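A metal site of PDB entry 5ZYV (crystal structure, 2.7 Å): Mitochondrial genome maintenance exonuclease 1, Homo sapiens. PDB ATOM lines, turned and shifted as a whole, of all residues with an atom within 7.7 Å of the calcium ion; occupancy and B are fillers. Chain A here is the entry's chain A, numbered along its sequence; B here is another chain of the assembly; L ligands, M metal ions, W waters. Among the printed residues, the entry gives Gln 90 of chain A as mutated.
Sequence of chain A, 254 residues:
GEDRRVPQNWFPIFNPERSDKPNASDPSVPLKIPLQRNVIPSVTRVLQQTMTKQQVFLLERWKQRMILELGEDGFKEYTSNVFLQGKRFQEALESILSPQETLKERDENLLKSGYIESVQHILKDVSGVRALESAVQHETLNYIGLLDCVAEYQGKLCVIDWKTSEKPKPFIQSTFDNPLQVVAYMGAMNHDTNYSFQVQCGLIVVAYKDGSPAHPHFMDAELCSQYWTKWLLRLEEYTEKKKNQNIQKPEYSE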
ATOM      1  N   GLY A  86       6.771  22.296   4.253  1.00  0.00           N
ATOM      2  CA  GLY A  86       6.232  23.382   3.453  1.00  0.00           C
ATOM      3  C   GLY A  86       7.100  23.727   2.261  1.00  0.00           C
ATOM      4  O   GLY A  86       6.592  24.041   1.181  1.00  0.00           O
ATOM      5  N   PHE A  89       6.990  20.669  -0.331  1.00  0.00           N
ATOM      6  CA  PHE A  89       5.733  20.658  -1.069  1.00  0.00           C
ATOM      7  C   PHE A  89       5.745  21.702  -2.180  1.00  0.00           C
ATOM      8  O   PHE A  89       5.317  21.436  -3.311  1.00  0.00           O
ATOM      9  CB  PHE A  89       4.574  20.903  -0.103  1.00  0.00           C
ATOM     10  CG  PHE A  89       3.263  21.154  -0.773  1.00  0.00           C
ATOM     11  CD1 PHE A  89       2.714  20.185  -1.599  1.00  0.00           C
ATOM     12  CD2 PHE A  89       2.591  22.340  -0.584  1.00  0.00           C
ATOM     13  CE1 PHE A  89       1.509  20.407  -2.218  1.00  0.00           C
ATOM     14  CE2 PHE A  89       1.386  22.567  -1.195  1.00  0.00           C
ATOM     15  CZ  PHE A  89       0.839  21.603  -2.013  1.00  0.00           C
ATOM     16  N   GLN A  90       6.306  22.849  -1.908  1.00  0.00           N
ATOM     17  CA  GLN A  90       6.374  23.795  -2.953  1.00  0.00           C
ATOM     18  C   GLN A  90       7.389  23.329  -3.974  1.00  0.00           C
ATOM     19  O   GLN A  90       7.125  23.356  -5.145  1.00  0.00           O
ATOM     20  CB  GLN A  90       6.771  25.110  -2.383  1.00  0.00           C
ATOM     21  CG  GLN A  90       7.390  25.997  -3.406  1.00  0.00           C
ATOM     22  CD  GLN A  90       8.384  26.895  -2.774  1.00  0.00           C
ATOM     23  OE1 GLN A  90       8.309  27.167  -1.579  1.00  0.00           O
ATOM     24  NE2 GLN A  90       9.314  27.355  -3.547  1.00  0.00           N
ATOM     25  N   LEU A 146       8.838  37.151  -2.704  1.00  0.00           N
ATOM     26  CA  LEU A 146       9.185  35.955  -3.485  1.00  0.00           C
ATOM     27  C   LEU A 146       7.938  35.074  -3.547  1.00  0.00           C
ATOM     28  O   LEU A 146       7.732  34.195  -2.703  1.00  0.00           O
ATOM     29  CB  LEU A 146      10.372  35.229  -2.867  1.00  0.00           C
ATOM     30  CG  LEU A 146      11.116  34.147  -3.643  1.00  0.00           C
ATOM     31  CD1 LEU A 146      11.647  34.742  -4.946  1.00  0.00           C
ATOM     32  CD2 LEU A 146      12.250  33.496  -2.816  1.00  0.00           C
ATOM     33  N   LEU A 147       7.097  35.302  -4.551  1.00  0.00           N
ATOM     34  CA  LEU A 147       5.859  34.552  -4.684  1.00  0.00           C
ATOM     35  C   LEU A 147       6.135  33.146  -5.204  1.00  0.00           C
ATOM     36  O   LEU A 147       7.167  32.873  -5.826  1.00  0.00           O
ATOM     37  CB  LEU A 147       4.885  35.284  -5.608  1.00  0.00           C
ATOM     38  CG  LEU A 147       5.393  35.690  -7.003  1.00  0.00           C
ATOM     39  CD1 LEU A 147       5.234  34.573  -8.038  1.00  0.00           C
ATOM     40  CD2 LEU A 147       4.698  36.955  -7.468  1.00  0.00           C
ATOM     41  N   ASP A 148       5.209  32.242  -4.914  1.00  0.00           N
ATOM     42  CA  ASP A 148       5.337  30.839  -5.309  1.00  0.00           C
ATOM     43  C   ASP A 148       5.297  30.644  -6.823  1.00  0.00           C
ATOM     44  O   ASP A 148       6.240  30.114  -7.413  1.00  0.00           O
ATOM     45  CB  ASP A 148       4.242  30.002  -4.645  1.00  0.00           C
ATOM     46  CG  ASP A 148       4.700  29.386  -3.333  1.00  0.00           C
ATOM     47  OD1 ASP A 148       5.914  29.407  -3.058  1.00  0.00           O
ATOM     48  OD2 ASP A 148       3.833  28.886  -2.579  1.00  0.00           O
ATOM     49  N   CYS A 149       4.216  31.080  -7.450  1.00  0.00           N
ATOM     50  CA  CYS A 149       4.063  30.928  -8.892  1.00  0.00           C
ATOM     51  C   CYS A 149       2.941  31.826  -9.377  1.00  0.00           C
ATOM     52  O   CYS A 149       2.130  32.336  -8.589  1.00  0.00           O
ATOM     53  CB  CYS A 149       3.806  29.468  -9.270  1.00  0.00           C
ATOM     54  SG  CYS A 149       2.070  29.049  -9.484  1.00  0.00           S
ATOM     55  N   ILE A 160      -0.646  32.390  -7.248  1.00  0.00           N
ATOM     56  CA  ILE A 160      -0.925  31.230  -6.408  1.00  0.00           C
ATOM     57  C   ILE A 160       0.130  31.154  -5.313  1.00  0.00           C
ATOM     58  O   ILE A 160       1.323  31.327  -5.584  1.00  0.00           O
ATOM     59  CB  ILE A 160      -0.954  29.944  -7.236  1.00  0.00           C
ATOM     60  CG1 ILE A 160      -1.943  30.060  -8.388  1.00  0.00           C
ATOM     61  CG2 ILE A 160      -1.308  28.753  -6.355  1.00  0.00           C
ATOM     62  CD1 ILE A 160      -1.961  28.843  -9.308  1.00  0.00           C
ATOM     63  N   ASP A 161      -0.316  30.827  -4.108  1.00  0.00           N
ATOM     64  CA  ASP A 161       0.575  30.667  -2.962  1.00  0.00           C
ATOM     65  C   ASP A 161       0.196  29.360  -2.266  1.00  0.00           C
ATOM     66  O   ASP A 161      -0.855  29.276  -1.630  1.00  0.00           O
ATOM     67  CB  ASP A 161       0.436  31.840  -1.993  1.00  0.00           C
ATOM     68  CG  ASP A 161       1.531  31.863  -0.942  1.00  0.00           C
ATOM     69  OD1 ASP A 161       2.190  30.821  -0.744  1.00  0.00           O
ATOM     70  OD2 ASP A 161       1.716  32.924  -0.303  1.00  0.00           O
ATOM     71  N   TRP A 162       1.052  28.349  -2.364  1.00  0.00           N
ATOM     72  CA  TRP A 162       0.765  27.057  -1.773  1.00  0.00           C
ATOM     73  C   TRP A 162       1.044  27.093  -0.275  1.00  0.00           C
ATOM     74  O   TRP A 162       2.038  27.675   0.175  1.00  0.00           O
ATOM     75  CB  TRP A 162       1.603  25.958  -2.420  1.00  0.00           C
ATOM     76  CG  TRP A 162       1.670  26.062  -3.909  1.00  0.00           C
ATOM     77  CD1 TRP A 162       2.690  26.592  -4.643  1.00  0.00           C
ATOM     78  CD2 TRP A 162       0.666  25.656  -4.850  1.00  0.00           C
ATOM     79  NE1 TRP A 162       2.399  26.522  -5.987  1.00  0.00           N
ATOM     80  CE2 TRP A 162       1.158  25.964  -6.134  1.00  0.00           C
ATOM     81  CE3 TRP A 162      -0.591  25.065  -4.724  1.00  0.00           C
ATOM     82  CZ2 TRP A 162       0.433  25.684  -7.299  1.00  0.00           C
ATOM     83  CZ3 TRP A 162      -1.315  24.791  -5.881  1.00  0.00           C
ATOM     84  CH2 TRP A 162      -0.798  25.107  -7.149  1.00  0.00           C
ATOM     85  N   LYS A 163       0.156  26.482   0.504  1.00  0.00           N
ATOM     86  CA  LYS A 163       0.323  26.364   1.947  1.00  0.00           C
ATOM     87  C   LYS A 163       0.140  24.921   2.369  1.00  0.00           C
ATOM     88  O   LYS A 163      -0.671  24.187   1.787  1.00  0.00           O
ATOM     89  CB  LYS A 163      -0.662  27.258   2.707  1.00  0.00           C
ATOM     90  CG  LYS A 163      -0.150  28.654   3.019  1.00  0.00           C
ATOM     91  CD  LYS A 163      -0.203  29.555   1.805  1.00  0.00           C
ATOM     92  CE  LYS A 163       0.084  31.011   2.169  1.00  0.00           C
ATOM     93  NZ  LYS A 163       1.429  31.188   2.780  1.00  0.00           N
ATOM     94  N   THR A 164       0.912  24.503   3.372  1.00  0.00           N
ATOM     95  CA  THR A 164       0.683  23.258   4.080  1.00  0.00           C
ATOM     96  C   THR A 164       0.129  23.588   5.457  1.00  0.00           C
ATOM     97  O   THR A 164       0.531  24.579   6.076  1.00  0.00           O
ATOM     98  CB  THR A 164       1.973  22.445   4.238  1.00  0.00           C
ATOM     99  OG1 THR A 164       2.971  23.236   4.902  1.00  0.00           O
ATOM    100  CG2 THR A 164       2.503  22.011   2.882  1.00  0.00           C
ATOM    101  N   GLN A 181      -0.440  38.655   2.304  1.00  0.00           N
ATOM    102  CA  GLN A 181       0.799  38.184   1.695  1.00  0.00           C
ATOM    103  C   GLN A 181       0.649  38.023   0.188  1.00  0.00           C
ATOM    104  O   GLN A 181       1.572  38.325  -0.568  1.00  0.00           O
ATOM    105  CB  GLN A 181       1.221  36.866   2.349  1.00  0.00           C
ATOM    106  CG  GLN A 181       2.436  36.221   1.722  1.00  0.00           C
ATOM    107  CD  GLN A 181       2.843  34.936   2.428  1.00  0.00           C
ATOM    108  OE1 GLN A 181       2.437  34.680   3.561  1.00  0.00           O
ATOM    109  NE2 GLN A 181       3.663  34.134   1.764  1.00  0.00           N
ATOM    110  N   TYR A 185       2.283  40.435  -2.933  1.00  0.00           N
ATOM    111  CA  TYR A 185       3.084  39.902  -4.026  1.00  0.00           C
ATOM    112  C   TYR A 185       2.602  40.424  -5.371  1.00  0.00           C
ATOM    113  O   TYR A 185       3.413  40.741  -6.240  1.00  0.00           O
ATOM    114  CB  TYR A 185       3.049  38.370  -3.996  1.00  0.00           C
ATOM    115  CG  TYR A 185       3.872  37.745  -2.893  1.00  0.00           C
ATOM    116  CD1 TYR A 185       4.920  38.448  -2.300  1.00  0.00           C
ATOM    117  CD2 TYR A 185       3.608  36.459  -2.452  1.00  0.00           C
ATOM    118  CE1 TYR A 185       5.680  37.874  -1.293  1.00  0.00           C
ATOM    119  CE2 TYR A 185       4.350  35.879  -1.438  1.00  0.00           C
ATOM    120  CZ  TYR A 185       5.388  36.593  -0.862  1.00  0.00           C
ATOM    121  OH  TYR A 185       6.134  36.019   0.135  1.00  0.00           O
ATOM    122  N   VAL A 205      -4.068  28.217  -1.504  1.00  0.00           N
ATOM    123  CA  VAL A 205      -4.405  26.802  -1.495  1.00  0.00           C
ATOM    124  C   VAL A 205      -3.795  26.220  -0.224  1.00  0.00           C
ATOM    125  O   VAL A 205      -2.603  26.427   0.043  1.00  0.00           O
ATOM    126  CB  VAL A 205      -3.839  26.066  -2.726  1.00  0.00           C
ATOM    127  CG1 VAL A 205      -4.163  24.587  -2.643  1.00  0.00           C
ATOM    128  CG2 VAL A 205      -4.403  26.675  -3.996  1.00  0.00           C
ATOM    129  P    DA B   4       9.353  36.896   1.312  1.00  0.00           P
ATOM    130  OP1  DA B   4       8.497  37.487   0.270  1.00  0.00           O
ATOM    131  OP2  DA B   4       9.328  37.435   2.689  1.00  0.00           O
ATOM    132  O5'  DA B   4       8.993  35.356   1.390  1.00  0.00           O
ATOM    133  C5'  DA B   4       9.244  34.657   2.570  1.00  0.00           C
ATOM    134  C4'  DA B   4       9.271  33.179   2.320  1.00  0.00           C
ATOM    135  O4'  DA B   4      10.641  32.722   2.291  1.00  0.00           O
ATOM    136  C3'  DA B   4       8.554  32.367   3.391  1.00  0.00           C
ATOM    137  O3'  DA B   4       7.273  32.007   2.912  1.00  0.00           O
ATOM    138  C2'  DA B   4       9.460  31.157   3.591  1.00  0.00           C
ATOM    139  C1'  DA B   4      10.843  31.702   3.239  1.00  0.00           C
ATOM    140  N9   DA B   4      11.587  32.253   4.373  1.00  0.00           N
ATOM    141  C8   DA B   4      11.297  33.397   5.072  1.00  0.00           C
ATOM    142  N7   DA B   4      12.152  33.651   6.045  1.00  0.00           N
ATOM    143  C5   DA B   4      13.061  32.607   5.972  1.00  0.00           C
ATOM    144  C6   DA B   4      14.208  32.301   6.724  1.00  0.00           C
ATOM    145  N6   DA B   4      14.647  33.042   7.744  1.00  0.00           N
ATOM    146  N1   DA B   4      14.896  31.179   6.385  1.00  0.00           N
ATOM    147  C2   DA B   4      14.448  30.435   5.368  1.00  0.00           C
ATOM    148  N3   DA B   4      13.388  30.620   4.587  1.00  0.00           N
ATOM    149  C4   DA B   4      12.729  31.743   4.944  1.00  0.00           C
ATOM    150  P    DA B   5       6.072  31.718   3.935  1.00  0.00           P
ATOM    151  OP1  DA B   5       4.802  31.920   3.206  1.00  0.00           O
ATOM    152  OP2  DA B   5       6.334  32.486   5.176  1.00  0.00           O
ATOM    153  O5'  DA B   5       6.221  30.160   4.241  1.00  0.00           O
ATOM    154  C5'  DA B   5       6.467  29.255   3.172  1.00  0.00           C
ATOM    155  C4'  DA B   5       7.098  27.973   3.691  1.00  0.00           C
ATOM    156  O4'  DA B   5       8.460  28.247   4.096  1.00  0.00           O
ATOM    157  C3'  DA B   5       6.409  27.402   4.917  1.00  0.00           C
ATOM    158  O3'  DA B   5       5.439  26.465   4.509  1.00  0.00           O
ATOM    159  C2'  DA B   5       7.549  26.729   5.675  1.00  0.00           C
ATOM    160  C1'  DA B   5       8.752  27.610   5.326  1.00  0.00           C
ATOM    161  N9   DA B   5       9.053  28.629   6.321  1.00  0.00           N
ATOM    162  C8   DA B   5       8.191  29.551   6.855  1.00  0.00           C
ATOM    163  N7   DA B   5       8.743  30.357   7.724  1.00  0.00           N
ATOM    164  C5   DA B   5      10.068  29.938   7.761  1.00  0.00           C
ATOM    165  C6   DA B   5      11.185  30.393   8.501  1.00  0.00           C
ATOM    166  N6   DA B   5      11.133  31.405   9.370  1.00  0.00           N
ATOM    167  N1   DA B   5      12.365  29.762   8.298  1.00  0.00           N
ATOM    168  C2   DA B   5      12.407  28.742   7.425  1.00  0.00           C
ATOM    169  N3   DA B   5      11.430  28.236   6.686  1.00  0.00           N
ATOM    170  C4   DA B   5      10.275  28.876   6.903  1.00  0.00           C
ATOM    171  P    DC B   6       3.885  26.803   4.661  1.00  0.00           P
ATOM    172  OP1  DC B   6       3.125  25.697   4.021  1.00  0.00           O
ATOM    173  OP2  DC B   6       3.658  28.198   4.230  1.00  0.00           O
ATOM    174  O5'  DC B   6       3.641  26.753   6.236  1.00  0.00           O
ATOM    175  C5'  DC B   6       3.926  25.568   6.944  1.00  0.00           C
ATOM    176  C4'  DC B   6       3.745  25.790   8.423  1.00  0.00           C
ATOM    177  O4'  DC B   6       4.675  26.781   8.898  1.00  0.00           O
ATOM    178  C3'  DC B   6       2.353  26.289   8.844  1.00  0.00           C
ATOM    179  O3'  DC B   6       1.694  25.288   9.611  1.00  0.00           O
ATOM    180  C2'  DC B   6       2.633  27.558   9.672  1.00  0.00           C
ATOM    181  C1'  DC B   6       4.109  27.419  10.000  1.00  0.00           C
ATOM    182  N1   DC B   6       4.833  28.718  10.250  1.00  0.00           N
ATOM    183  C2   DC B   6       4.916  29.694   9.243  1.00  0.00           C
ATOM    184  O2   DC B   6       4.370  29.487   8.151  1.00  0.00           O
ATOM    185  N3   DC B   6       5.583  30.840   9.502  1.00  0.00           N
ATOM    186  C4   DC B   6       6.159  31.030  10.695  1.00  0.00           C
ATOM    187  N4   DC B   6       6.813  32.185  10.891  1.00  0.00           N
ATOM    188  C5   DC B   6       6.096  30.053  11.724  1.00  0.00           C
ATOM    189  C6   DC B   6       5.433  28.917  11.458  1.00  0.00           C
HETATM  190  C1  LIG L   1       6.400  31.608  -0.573  1.00  0.00           C
HETATM  191  O1  LIG L   1       5.727  30.565  -0.526  1.00  0.00           O
HETATM  192  O2  LIG L   1       5.767  32.670  -0.394  1.00  0.00           O
HETATM  193  C2  LIG L   1       7.889  31.581  -0.829  1.00  0.00           C
HETATM  194 CA    CA M   1       3.760  29.328  -0.195  1.00  0.00          CA
HETATM  195  O   HOH W   1       3.469  29.776   2.048  1.00  0.00           O
HETATM  196  O   HOH W   2       4.878  27.317  -0.138  1.00  0.00           O
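The side-chain carboxylate (OD2) of Asp 161 lies within salt-bridge range of the side-chain amino group (NZ) of Lys 163 (3.5 Å).
The side-chain amide nitrogen (NE2) of Gln 181 lies within hydrogen-bond range of the side-chain carboxylate (OD2) of Asp 161 (3.1 Å).
The backbone NH (N) of Val 205 sits at hydrogen-bond distance from the backbone carbonyl oxygen (O) of Asp 161.
Within 4 Å of the calcium ion: Asp 148, Asp 161 and Trp 162.
The nearest printed residue that does not touch the calcium ion is Lys 163 (4.2 Å).
The calcium ion is bound by the side-chain carboxylate of Asp 161 (2.2 Å), water W2 (2.3 Å), water W1 (2.3 Å), an oxygen (O1) of the ligand (2.3 Å), the backbone carbonyl oxygen of Trp 162 (2.4 Å) and the side-chain carboxylate of Asp 148 (2.4 Å).
Water W1 lies within hydrogen-bond range of the side-chain amino group of Lys 163, OP2 of DC 6 of chain B and OP1 of DA 5 of chain B.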
